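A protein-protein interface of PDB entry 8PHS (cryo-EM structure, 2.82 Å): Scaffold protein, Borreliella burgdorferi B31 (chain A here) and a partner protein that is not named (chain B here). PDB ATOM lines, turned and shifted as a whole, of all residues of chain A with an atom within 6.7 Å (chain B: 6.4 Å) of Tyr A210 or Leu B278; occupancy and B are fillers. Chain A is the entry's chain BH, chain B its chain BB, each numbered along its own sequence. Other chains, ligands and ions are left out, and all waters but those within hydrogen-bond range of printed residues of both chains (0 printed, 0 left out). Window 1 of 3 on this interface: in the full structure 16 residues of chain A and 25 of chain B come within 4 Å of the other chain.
O of Val B20 sits at hydrogen-bond distance from NH1 of Arg A213 (3.1 Å).
The guanidinium group (NE) of Arg A213 is in salt-bridge range of the side-chain carboxylate (OD1) of Asp B22, 3.8 Å away.
OD1 of Asp B36 lies within salt-bridge range of NH1 of Arg A214 (3.0 Å).
O of Lys B275 is in hydrogen-bond range of OG of Ser A207 (3.3 Å).
The backbone carbonyl oxygen of Pro B279 lies within hydrogen-bond range of the side-chain hydroxyl of Tyr A210 (3.5 Å).
The side-chain hydroxyl (OG) of Ser B274 lies close to the backbone NH (N) of Tyr B276 (3.1 Å).
The backbone carbonyl oxygen (O) of Leu B278 lies within hydrogen-bond range of the side-chain hydroxyl (OG1) of Thr B280 (3.3 Å).
Ser A207 touches Tyr B276 (OG to CD1, 3.4 Å).
CD1 of Ile B17 touches OH of Tyr A210, 3.5 Å away.
Tyr A210 touches Leu B278 (CD1 to CD1, 3.5 Å).
CZ of Tyr B26 touches CG of Arg A214, 3.6 Å away.
Tyr A210 touches just these residues of chain B: Ile B17 (3.5 Å), Leu B278 (3.5 Å) and Pro B279 (3.5 Å).
Of chain A, only Tyr A210 (3.5 Å) comes within 4 Å of Leu B278.
Printed residues of chain A within 4 Å of Asp B22: Arg A213.
Printed residues of chain B within 4 Å of Arg A213: Val B20 (2.3 Å) and Asp B22 (3.8 Å).
Of the printed residues of chain A, Pro B279 touches Tyr A210.
Pro B23 touches none of the printed residues of chain A.
The nearest residue of chain B that does not touch Tyr A210 is Tyr B26 (4.7 Å).
The nearest residue of chain A that does not touch Leu B278 is Ile A206 (6.3 Å).
Printed residues of chain B that touch a printed residue of chain A: Ile B17, Val B20, Asp B22, Tyr B26, Asp B36, Lys B275, Tyr B276, Leu B278 and Pro B279.
Hydrophobic or aromatic side chains of chain B within 4 Å of the printed part of chain A: Ile B17, Tyr B26, Tyr B276 and Leu B278.
Printed residues of chain A that touch a printed residue of chain B: Ser A207, Tyr A210, Arg A213 and Arg A214.
Among the printed residues, 9 pairs touch across the chains.
Among the printed residues, Asp or Glu carboxylates within 4 Å of a Lys or Arg side-chain nitrogen of the other chain: Arg A213 with Asp B22 and Arg A214 with Asp B36.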
ATOM      1  N   SER A 188      17.336  -5.217  -4.985  1.00  0.00           N
ATOM      2  CA  SER A 188      15.980  -5.632  -5.311  1.00  0.00           C
ATOM      3  C   SER A 188      15.617  -6.880  -4.522  1.00  0.00           C
ATOM      4  O   SER A 188      16.458  -7.759  -4.313  1.00  0.00           O
ATOM      5  CB  SER A 188      15.832  -5.903  -6.814  1.00  0.00           C
ATOM      6  OG  SER A 188      14.525  -6.351  -7.126  1.00  0.00           O
ATOM      7  N   ALA A 205      14.757  -1.199  -1.611  1.00  0.00           N
ATOM      8  CA  ALA A 205      14.625  -2.455  -2.340  1.00  0.00           C
ATOM      9  C   ALA A 205      13.188  -2.686  -2.787  1.00  0.00           C
ATOM     10  O   ALA A 205      12.949  -3.192  -3.888  1.00  0.00           O
ATOM     11  CB  ALA A 205      15.111  -3.617  -1.478  1.00  0.00           C
ATOM     12  N   ILE A 206      12.217  -2.333  -1.942  1.00  0.00           N
ATOM     13  CA  ILE A 206      10.814  -2.480  -2.326  1.00  0.00           C
ATOM     14  C   ILE A 206      10.495  -1.604  -3.533  1.00  0.00           C
ATOM     15  O   ILE A 206       9.824  -2.041  -4.480  1.00  0.00           O
ATOM     16  CB  ILE A 206       9.893  -2.154  -1.135  1.00  0.00           C
ATOM     17  CG1 ILE A 206      10.032  -3.217  -0.047  1.00  0.00           C
ATOM     18  CG2 ILE A 206       8.448  -2.048  -1.589  1.00  0.00           C
ATOM     19  CD1 ILE A 206       9.199  -2.934   1.178  1.00  0.00           C
ATOM     20  N   SER A 207      10.964  -0.355  -3.517  1.00  0.00           N
ATOM     21  CA  SER A 207      10.720   0.537  -4.648  1.00  0.00           C
ATOM     22  C   SER A 207      11.367   0.006  -5.922  1.00  0.00           C
ATOM     23  O   SER A 207      10.757   0.031  -7.002  1.00  0.00           O
ATOM     24  CB  SER A 207      11.234   1.940  -4.330  1.00  0.00           C
ATOM     25  OG  SER A 207      10.650   2.439  -3.141  1.00  0.00           O
ATOM     26  N   ASN A 208      12.606  -0.481  -5.816  1.00  0.00           N
ATOM     27  CA  ASN A 208      13.282  -1.042  -6.981  1.00  0.00           C
ATOM     28  C   ASN A 208      12.545  -2.266  -7.509  1.00  0.00           C
ATOM     29  O   ASN A 208      12.441  -2.461  -8.725  1.00  0.00           O
ATOM     30  CB  ASN A 208      14.726  -1.393  -6.629  1.00  0.00           C
ATOM     31  CG  ASN A 208      15.559  -0.171  -6.305  1.00  0.00           C
ATOM     32  OD1 ASN A 208      15.097   0.961  -6.440  1.00  0.00           O
ATOM     33  ND2 ASN A 208      16.792  -0.394  -5.870  1.00  0.00           N
ATOM     34  N   THR A 209      12.033  -3.106  -6.606  1.00  0.00           N
ATOM     35  CA  THR A 209      11.267  -4.273  -7.026  1.00  0.00           C
ATOM     36  C   THR A 209      10.002  -3.863  -7.767  1.00  0.00           C
ATOM     37  O   THR A 209       9.651  -4.464  -8.789  1.00  0.00           O
ATOM     38  CB  THR A 209      10.921  -5.136  -5.812  1.00  0.00           C
ATOM     39  OG1 THR A 209      12.123  -5.678  -5.252  1.00  0.00           O
ATOM     40  CG2 THR A 209       9.996  -6.277  -6.207  1.00  0.00           C
ATOM     41  N   TYR A 210       9.304  -2.840  -7.269  1.00  0.00           N
ATOM     42  CA  TYR A 210       8.110  -2.365  -7.964  1.00  0.00           C
ATOM     43  C   TYR A 210       8.451  -1.850  -9.358  1.00  0.00           C
ATOM     44  O   TYR A 210       7.737  -2.138 -10.330  1.00  0.00           O
ATOM     45  CB  TYR A 210       7.421  -1.273  -7.147  1.00  0.00           C
ATOM     46  CG  TYR A 210       6.460  -1.795  -6.105  1.00  0.00           C
ATOM     47  CD1 TYR A 210       5.557  -2.803  -6.410  1.00  0.00           C
ATOM     48  CD2 TYR A 210       6.443  -1.268  -4.821  1.00  0.00           C
ATOM     49  CE1 TYR A 210       4.672  -3.279  -5.463  1.00  0.00           C
ATOM     50  CE2 TYR A 210       5.562  -1.736  -3.868  1.00  0.00           C
ATOM     51  CZ  TYR A 210       4.678  -2.741  -4.195  1.00  0.00           C
ATOM     52  OH  TYR A 210       3.799  -3.213  -3.249  1.00  0.00           O
ATOM     53  N   LYS A 211       9.541  -1.088  -9.477  1.00  0.00           N
ATOM     54  CA  LYS A 211       9.941  -0.580 -10.787  1.00  0.00           C
ATOM     55  C   LYS A 211      10.291  -1.719 -11.741  1.00  0.00           C
ATOM     56  O   LYS A 211       9.898  -1.703 -12.916  1.00  0.00           O
ATOM     57  CB  LYS A 211      11.122   0.377 -10.639  1.00  0.00           C
ATOM     58  CG  LYS A 211      11.699   0.858 -11.957  1.00  0.00           C
ATOM     59  CD  LYS A 211      12.893   1.769 -11.734  1.00  0.00           C
ATOM     60  CE  LYS A 211      13.469   2.252 -13.052  1.00  0.00           C
ATOM     61  NZ  LYS A 211      14.592   3.208 -12.847  1.00  0.00           N
ATOM     62  N   GLN A 212      11.025  -2.721 -11.249  1.00  0.00           N
ATOM     63  CA  GLN A 212      11.387  -3.857 -12.089  1.00  0.00           C
ATOM     64  C   GLN A 212      10.155  -4.641 -12.520  1.00  0.00           C
ATOM     65  O   GLN A 212      10.082  -5.121 -13.655  1.00  0.00           O
ATOM     66  CB  GLN A 212      12.369  -4.764 -11.350  1.00  0.00           C
ATOM     67  CG  GLN A 212      13.739  -4.145 -11.139  1.00  0.00           C
ATOM     68  CD  GLN A 212      14.667  -5.041 -10.345  1.00  0.00           C
ATOM     69  OE1 GLN A 212      14.278  -6.122  -9.905  1.00  0.00           O
ATOM     70  NE2 GLN A 212      15.904  -4.595 -10.159  1.00  0.00           N
ATOM     71  N   ARG A 213       9.180  -4.791 -11.622  1.00  0.00           N
ATOM     72  CA  ARG A 213       7.946  -5.482 -11.983  1.00  0.00           C
ATOM     73  C   ARG A 213       7.171  -4.714 -13.044  1.00  0.00           C
ATOM     74  O   ARG A 213       6.597  -5.318 -13.956  1.00  0.00           O
ATOM     75  CB  ARG A 213       7.089  -5.709 -10.740  1.00  0.00           C
ATOM     76  CG  ARG A 213       7.670  -6.725  -9.775  1.00  0.00           C
ATOM     77  CD  ARG A 213       6.635  -7.755  -9.379  1.00  0.00           C
ATOM     78  NE  ARG A 213       5.508  -7.141  -8.691  1.00  0.00           N
ATOM     79  CZ  ARG A 213       4.401  -7.782  -8.345  1.00  0.00           C
ATOM     80  NH1 ARG A 213       4.233  -9.065  -8.619  1.00  0.00           N
ATOM     81  NH2 ARG A 213       3.440  -7.120  -7.710  1.00  0.00           N
ATOM     82  N   ARG A 214       7.139  -3.383 -12.943  1.00  0.00           N
ATOM     83  CA  ARG A 214       6.490  -2.587 -13.983  1.00  0.00           C
ATOM     84  C   ARG A 214       7.188  -2.761 -15.327  1.00  0.00           C
ATOM     85  O   ARG A 214       6.530  -2.914 -16.368  1.00  0.00           O
ATOM     86  CB  ARG A 214       6.471  -1.115 -13.581  1.00  0.00           C
ATOM     87  CG  ARG A 214       5.827  -0.197 -14.602  1.00  0.00           C
ATOM     88  CD  ARG A 214       5.963   1.249 -14.174  1.00  0.00           C
ATOM     89  NE  ARG A 214       7.360   1.661 -14.121  1.00  0.00           N
ATOM     90  CZ  ARG A 214       7.816   2.674 -13.398  1.00  0.00           C
ATOM     91  NH1 ARG A 214       7.011   3.395 -12.635  1.00  0.00           N
ATOM     92  NH2 ARG A 214       9.112   2.968 -13.437  1.00  0.00           N
ATOM     93  N   ILE A 215       8.523  -2.741 -15.323  1.00  0.00           N
ATOM     94  CA  ILE A 215       9.272  -2.921 -16.563  1.00  0.00           C
ATOM     95  C   ILE A 215       8.996  -4.296 -17.159  1.00  0.00           C
ATOM     96  O   ILE A 215       8.798  -4.435 -18.373  1.00  0.00           O
ATOM     97  CB  ILE A 215      10.776  -2.698 -16.316  1.00  0.00           C
ATOM     98  CG1 ILE A 215      11.057  -1.217 -16.060  1.00  0.00           C
ATOM     99  CG2 ILE A 215      11.593  -3.198 -17.493  1.00  0.00           C
ATOM    100  CD1 ILE A 215      12.501  -0.919 -15.739  1.00  0.00           C
ATOM    101  N   ILE B  17       5.805 -10.095  -0.924  1.00  0.00           N
ATOM    102  CA  ILE B  17       5.603  -8.953  -1.808  1.00  0.00           C
ATOM    103  C   ILE B  17       5.439  -9.376  -3.262  1.00  0.00           C
ATOM    104  O   ILE B  17       4.854  -8.632  -4.058  1.00  0.00           O
ATOM    105  CB  ILE B  17       6.762  -7.949  -1.654  1.00  0.00           C
ATOM    106  CG1 ILE B  17       6.362  -6.576  -2.196  1.00  0.00           C
ATOM    107  CG2 ILE B  17       8.013  -8.456  -2.351  1.00  0.00           C
ATOM    108  CD1 ILE B  17       5.175  -5.967  -1.491  1.00  0.00           C
ATOM    109  N   VAL B  20       1.557  -9.911  -4.926  1.00  0.00           N
ATOM    110  CA  VAL B  20       0.621  -8.813  -5.138  1.00  0.00           C
ATOM    111  C   VAL B  20       0.538  -8.528  -6.630  1.00  0.00           C
ATOM    112  O   VAL B  20       1.564  -8.368  -7.299  1.00  0.00           O
ATOM    113  CB  VAL B  20       1.055  -7.561  -4.357  1.00  0.00           C
ATOM    114  CG1 VAL B  20       0.062  -6.434  -4.575  1.00  0.00           C
ATOM    115  CG2 VAL B  20       1.187  -7.880  -2.876  1.00  0.00           C
ATOM    116  N   ASP B  22      -0.092  -6.718 -10.257  1.00  0.00           N
ATOM    117  CA  ASP B  22       0.257  -5.415 -10.793  1.00  0.00           C
ATOM    118  C   ASP B  22      -0.991  -4.541 -10.920  1.00  0.00           C
ATOM    119  O   ASP B  22      -2.095  -5.049 -11.135  1.00  0.00           O
ATOM    120  CB  ASP B  22       0.926  -5.555 -12.157  1.00  0.00           C
ATOM    121  CG  ASP B  22       2.266  -6.258 -12.079  1.00  0.00           C
ATOM    122  OD1 ASP B  22       3.144  -5.789 -11.326  1.00  0.00           O
ATOM    123  OD2 ASP B  22       2.443  -7.278 -12.777  1.00  0.00           O
ATOM    124  N   PRO B  23      -0.844  -3.225 -10.775  1.00  0.00           N
ATOM    125  CA  PRO B  23      -1.992  -2.332 -10.970  1.00  0.00           C
ATOM    126  C   PRO B  23      -2.505  -2.390 -12.400  1.00  0.00           C
ATOM    127  O   PRO B  23      -1.741  -2.559 -13.353  1.00  0.00           O
ATOM    128  CB  PRO B  23      -1.425  -0.946 -10.637  1.00  0.00           C
ATOM    129  CG  PRO B  23      -0.205  -1.217  -9.816  1.00  0.00           C
ATOM    130  CD  PRO B  23       0.360  -2.491 -10.354  1.00  0.00           C
ATOM    131  N   MET B  25      -3.767   0.121 -13.892  1.00  0.00           N
ATOM    132  CA  MET B  25      -3.537   1.409 -14.531  1.00  0.00           C
ATOM    133  C   MET B  25      -2.348   1.380 -15.479  1.00  0.00           C
ATOM    134  O   MET B  25      -2.198   2.296 -16.293  1.00  0.00           O
ATOM    135  CB  MET B  25      -3.324   2.492 -13.474  1.00  0.00           C
ATOM    136  CG  MET B  25      -2.037   2.330 -12.693  1.00  0.00           C
ATOM    137  SD  MET B  25      -1.827   3.590 -11.427  1.00  0.00           S
ATOM    138  CE  MET B  25      -0.312   3.029 -10.662  1.00  0.00           C
ATOM    139  N   TYR B  26      -1.500   0.353 -15.391  1.00  0.00           N
ATOM    140  CA  TYR B  26      -0.367   0.240 -16.300  1.00  0.00           C
ATOM    141  C   TYR B  26      -0.806   0.020 -17.741  1.00  0.00           C
ATOM    142  O   TYR B  26      -0.029   0.295 -18.662  1.00  0.00           O
ATOM    143  CB  TYR B  26       0.546  -0.904 -15.860  1.00  0.00           C
ATOM    144  CG  TYR B  26       1.410  -0.590 -14.662  1.00  0.00           C
ATOM    145  CD1 TYR B  26       1.529   0.707 -14.186  1.00  0.00           C
ATOM    146  CD2 TYR B  26       2.105  -1.596 -14.005  1.00  0.00           C
ATOM    147  CE1 TYR B  26       2.319   0.994 -13.091  1.00  0.00           C
ATOM    148  CE2 TYR B  26       2.895  -1.319 -12.909  1.00  0.00           C
ATOM    149  CZ  TYR B  26       3.000  -0.023 -12.456  1.00  0.00           C
ATOM    150  OH  TYR B  26       3.787   0.257 -11.364  1.00  0.00           O
ATOM    151  N   ASP B  36       9.567   7.652 -12.604  1.00  0.00           N
ATOM    152  CA  ASP B  36       9.454   7.836 -11.165  1.00  0.00           C
ATOM    153  C   ASP B  36      10.264   9.036 -10.688  1.00  0.00           C
ATOM    154  O   ASP B  36      11.260   9.431 -11.302  1.00  0.00           O
ATOM    155  CB  ASP B  36       9.918   6.580 -10.428  1.00  0.00           C
ATOM    156  CG  ASP B  36       8.873   5.485 -10.427  1.00  0.00           C
ATOM    157  OD1 ASP B  36       7.749   5.733 -10.912  1.00  0.00           O
ATOM    158  OD2 ASP B  36       9.174   4.375  -9.942  1.00  0.00           O
ATOM    159  N   TYR B 119      -1.313  -8.102   5.194  1.00  0.00           N
ATOM    160  CA  TYR B 119      -0.589  -7.126   4.392  1.00  0.00           C
ATOM    161  C   TYR B 119      -0.901  -7.287   2.912  1.00  0.00           C
ATOM    162  O   TYR B 119      -1.092  -6.292   2.205  1.00  0.00           O
ATOM    163  CB  TYR B 119       0.914  -7.255   4.636  1.00  0.00           C
ATOM    164  CG  TYR B 119       1.740  -6.293   3.817  1.00  0.00           C
ATOM    165  CD1 TYR B 119       1.816  -4.950   4.155  1.00  0.00           C
ATOM    166  CD2 TYR B 119       2.431  -6.725   2.693  1.00  0.00           C
ATOM    167  CE1 TYR B 119       2.564  -4.067   3.405  1.00  0.00           C
ATOM    168  CE2 TYR B 119       3.180  -5.848   1.937  1.00  0.00           C
ATOM    169  CZ  TYR B 119       3.242  -4.521   2.297  1.00  0.00           C
ATOM    170  OH  TYR B 119       3.989  -3.647   1.544  1.00  0.00           O
ATOM    171  N   SER B 123      -2.673  -4.358   0.791  1.00  0.00           N
ATOM    172  CA  SER B 123      -1.954  -3.786  -0.339  1.00  0.00           C
ATOM    173  C   SER B 123      -2.781  -3.863  -1.612  1.00  0.00           C
ATOM    174  O   SER B 123      -2.799  -2.915  -2.404  1.00  0.00           O
ATOM    175  CB  SER B 123      -0.616  -4.501  -0.526  1.00  0.00           C
ATOM    176  OG  SER B 123       0.225  -4.309   0.598  1.00  0.00           O
ATOM    177  N   ILE B 126      -5.431  -1.142  -1.423  1.00  0.00           N
ATOM    178  CA  ILE B 126      -4.841   0.179  -1.618  1.00  0.00           C
ATOM    179  C   ILE B 126      -4.474   0.390  -3.083  1.00  0.00           C
ATOM    180  O   ILE B 126      -4.620   1.492  -3.622  1.00  0.00           O
ATOM    181  CB  ILE B 126      -3.629   0.362  -0.689  1.00  0.00           C
ATOM    182  CG1 ILE B 126      -4.085   0.392   0.770  1.00  0.00           C
ATOM    183  CG2 ILE B 126      -2.879   1.638  -1.025  1.00  0.00           C
ATOM    184  CD1 ILE B 126      -2.953   0.356   1.762  1.00  0.00           C
ATOM    185  N   ILE B 127      -3.997  -0.663  -3.751  1.00  0.00           N
ATOM    186  CA  ILE B 127      -3.673  -0.562  -5.173  1.00  0.00           C
ATOM    187  C   ILE B 127      -4.928  -0.270  -5.985  1.00  0.00           C
ATOM    188  O   ILE B 127      -4.903   0.537  -6.926  1.00  0.00           O
ATOM    189  CB  ILE B 127      -2.967  -1.845  -5.649  1.00  0.00           C
ATOM    190  CG1 ILE B 127      -1.518  -1.862  -5.161  1.00  0.00           C
ATOM    191  CG2 ILE B 127      -3.021  -1.964  -7.162  1.00  0.00           C
ATOM    192  CD1 ILE B 127      -0.718  -3.035  -5.667  1.00  0.00           C
ATOM    193  N   ILE B 130      -5.654   3.357  -5.578  1.00  0.00           N
ATOM    194  CA  ILE B 130      -4.729   4.173  -6.365  1.00  0.00           C
ATOM    195  C   ILE B 130      -5.133   4.176  -7.834  1.00  0.00           C
ATOM    196  O   ILE B 130      -5.071   5.212  -8.508  1.00  0.00           O
ATOM    197  CB  ILE B 130      -3.283   3.681  -6.176  1.00  0.00           C
ATOM    198  CG1 ILE B 130      -2.844   3.856  -4.722  1.00  0.00           C
ATOM    199  CG2 ILE B 130      -2.339   4.423  -7.105  1.00  0.00           C
ATOM    200  CD1 ILE B 130      -1.442   3.370  -4.449  1.00  0.00           C
ATOM    201  N   SER B 274       5.583   9.383  -7.574  1.00  0.00           N
ATOM    202  CA  SER B 274       6.616   9.155  -6.578  1.00  0.00           C
ATOM    203  C   SER B 274       7.014   7.686  -6.594  1.00  0.00           C
ATOM    204  O   SER B 274       6.178   6.805  -6.809  1.00  0.00           O
ATOM    205  CB  SER B 274       6.117   9.559  -5.193  1.00  0.00           C
ATOM    206  OG  SER B 274       6.940   9.016  -4.179  1.00  0.00           O
ATOM    207  N   LYS B 275       8.299   7.417  -6.377  1.00  0.00           N
ATOM    208  CA  LYS B 275       8.719   6.022  -6.347  1.00  0.00           C
ATOM    209  C   LYS B 275       8.220   5.292  -5.111  1.00  0.00           C
ATOM    210  O   LYS B 275       8.428   4.079  -5.000  1.00  0.00           O
ATOM    211  CB  LYS B 275      10.242   5.920  -6.451  1.00  0.00           C
ATOM    212  CG  LYS B 275      11.015   6.567  -5.321  1.00  0.00           C
ATOM    213  CD  LYS B 275      12.493   6.241  -5.453  1.00  0.00           C
ATOM    214  CE  LYS B 275      13.293   6.780  -4.285  1.00  0.00           C
ATOM    215  NZ  LYS B 275      14.705   6.317  -4.328  1.00  0.00           N
ATOM    216  N   TYR B 276       7.569   6.000  -4.188  1.00  0.00           N
ATOM    217  CA  TYR B 276       6.891   5.401  -3.048  1.00  0.00           C
ATOM    218  C   TYR B 276       5.374   5.428  -3.207  1.00  0.00           C
ATOM    219  O   TYR B 276       4.649   5.313  -2.214  1.00  0.00           O
ATOM    220  CB  TYR B 276       7.300   6.110  -1.758  1.00  0.00           C
ATOM    221  CG  TYR B 276       8.793   6.257  -1.586  1.00  0.00           C
ATOM    222  CD1 TYR B 276       9.608   5.144  -1.441  1.00  0.00           C
ATOM    223  CD2 TYR B 276       9.388   7.511  -1.567  1.00  0.00           C
ATOM    224  CE1 TYR B 276      10.971   5.274  -1.281  1.00  0.00           C
ATOM    225  CE2 TYR B 276      10.751   7.651  -1.410  1.00  0.00           C
ATOM    226  CZ  TYR B 276      11.538   6.530  -1.267  1.00  0.00           C
ATOM    227  OH  TYR B 276      12.897   6.663  -1.108  1.00  0.00           O
ATOM    228  N   MET B 277       4.881   5.592  -4.437  1.00  0.00           N
ATOM    229  CA  MET B 277       3.439   5.665  -4.658  1.00  0.00           C
ATOM    230  C   MET B 277       2.749   4.363  -4.273  1.00  0.00           C
ATOM    231  O   MET B 277       1.684   4.378  -3.647  1.00  0.00           O
ATOM    232  CB  MET B 277       3.148   6.008  -6.118  1.00  0.00           C
ATOM    233  CG  MET B 277       1.762   5.595  -6.584  1.00  0.00           C
ATOM    234  SD  MET B 277       1.472   5.950  -8.323  1.00  0.00           S
ATOM    235  CE  MET B 277       2.466   4.670  -9.084  1.00  0.00           C
ATOM    236  N   LEU B 278       3.334   3.228  -4.644  1.00  0.00           N
ATOM    237  CA  LEU B 278       2.740   1.943  -4.328  1.00  0.00           C
ATOM    238  C   LEU B 278       2.896   1.642  -2.837  1.00  0.00           C
ATOM    239  O   LEU B 278       3.786   2.184  -2.177  1.00  0.00           O
ATOM    240  CB  LEU B 278       3.377   0.851  -5.184  1.00  0.00           C
ATOM    241  CG  LEU B 278       2.920   0.893  -6.646  1.00  0.00           C
ATOM    242  CD1 LEU B 278       3.315  -0.369  -7.386  1.00  0.00           C
ATOM    243  CD2 LEU B 278       1.416   1.113  -6.733  1.00  0.00           C
ATOM    244  N   PRO B 279       2.030   0.788  -2.283  1.00  0.00           N
ATOM    245  CA  PRO B 279       2.020   0.583  -0.828  1.00  0.00           C
ATOM    246  C   PRO B 279       3.370   0.131  -0.289  1.00  0.00           C
ATOM    247  O   PRO B 279       4.059  -0.695  -0.890  1.00  0.00           O
ATOM    248  CB  PRO B 279       0.954  -0.500  -0.637  1.00  0.00           C
ATOM    249  CG  PRO B 279       0.041  -0.321  -1.787  1.00  0.00           C
ATOM    250  CD  PRO B 279       0.906   0.097  -2.938  1.00  0.00           C
ATOM    251  N   THR B 280       3.740   0.687   0.868  1.00  0.00           N
ATOM    252  CA  THR B 280       5.013   0.400   1.521  1.00  0.00           C
ATOM    253  C   THR B 280       4.760   0.243   3.017  1.00  0.00           C
ATOM    254  O   THR B 280       4.037   1.064   3.607  1.00  0.00           O
ATOM    255  CB  THR B 280       6.032   1.513   1.257  1.00  0.00           C
ATOM    256  OG1 THR B 280       6.273   1.620  -0.150  1.00  0.00           O
ATOM    257  CG2 THR B 280       7.346   1.235   1.972  1.00  0.00           C
ATOM    258  N   ILE B 297       0.475   1.090   6.531  1.00  0.00           N
ATOM    259  CA  ILE B 297       0.887   1.075   5.133  1.00  0.00           C
ATOM    260  C   ILE B 297       0.803   2.492   4.587  1.00  0.00           C
ATOM    261  O   ILE B 297      -0.209   3.176   4.776  1.00  0.00           O
ATOM    262  CB  ILE B 297       0.022   0.122   4.289  1.00  0.00           C
ATOM    263  CG1 ILE B 297       0.055  -1.290   4.871  1.00  0.00           C
ATOM    264  CG2 ILE B 297       0.509   0.099   2.857  1.00  0.00           C
ATOM    265  CD1 ILE B 297      -0.633  -2.320   4.009  1.00  0.00           C
ATOM    266  N   ASP B 298       1.859   2.927   3.903  1.00  0.00           N
ATOM    267  CA  ASP B 298       1.966   4.263   3.340  1.00  0.00           C
ATOM    268  C   ASP B 298       1.898   4.203   1.819  1.00  0.00           C
ATOM    269  O   ASP B 298       2.365   3.243   1.198  1.00  0.00           O
ATOM    270  CB  ASP B 298       3.283   4.930   3.753  1.00  0.00           C
ATOM    271  CG  ASP B 298       3.280   5.393   5.193  1.00  0.00           C
ATOM    272  OD1 ASP B 298       2.383   6.175   5.564  1.00  0.00           O
ATOM    273  OD2 ASP B 298       4.184   4.980   5.951  1.00  0.00           O
ATOM    274  N   PHE B 299       1.315   5.242   1.224  1.00  0.00           N
ATOM    275  CA  PHE B 299       1.331   5.395  -0.224  1.00  0.00           C
ATOM    276  C   PHE B 299       1.255   6.877  -0.567  1.00  0.00           C
ATOM    277  O   PHE B 299       0.956   7.718   0.282  1.00  0.00           O
ATOM    278  CB  PHE B 299       0.210   4.588  -0.898  1.00  0.00           C
ATOM    279  CG  PHE B 299      -1.177   4.978  -0.479  1.00  0.00           C
ATOM    280  CD1 PHE B 299      -1.683   4.591   0.750  1.00  0.00           C
ATOM    281  CD2 PHE B 299      -1.990   5.705  -1.331  1.00  0.00           C
ATOM    282  CE1 PHE B 299      -2.963   4.939   1.128  1.00  0.00           C
ATOM    283  CE2 PHE B 299      -3.271   6.056  -0.957  1.00  0.00           C
ATOM    284  CZ  PHE B 299      -3.759   5.670   0.273  1.00  0.00           C
ATOM    285  N   VAL B 300       1.576   7.196  -1.821  1.00  0.00           N
ATOM    286  CA  VAL B 300       1.681   8.575  -2.286  1.00  0.00           C
ATOM    287  C   VAL B 300       0.843   8.740  -3.545  1.00  0.00           C
ATOM    288  O   VAL B 300       0.851   7.872  -4.427  1.00  0.00           O
ATOM    289  CB  VAL B 300       3.146   8.980  -2.554  1.00  0.00           C
ATOM    290  CG1 VAL B 300       3.236  10.456  -2.897  1.00  0.00           C
ATOM    291  CG2 VAL B 300       4.021   8.655  -1.354  1.00  0.00           C
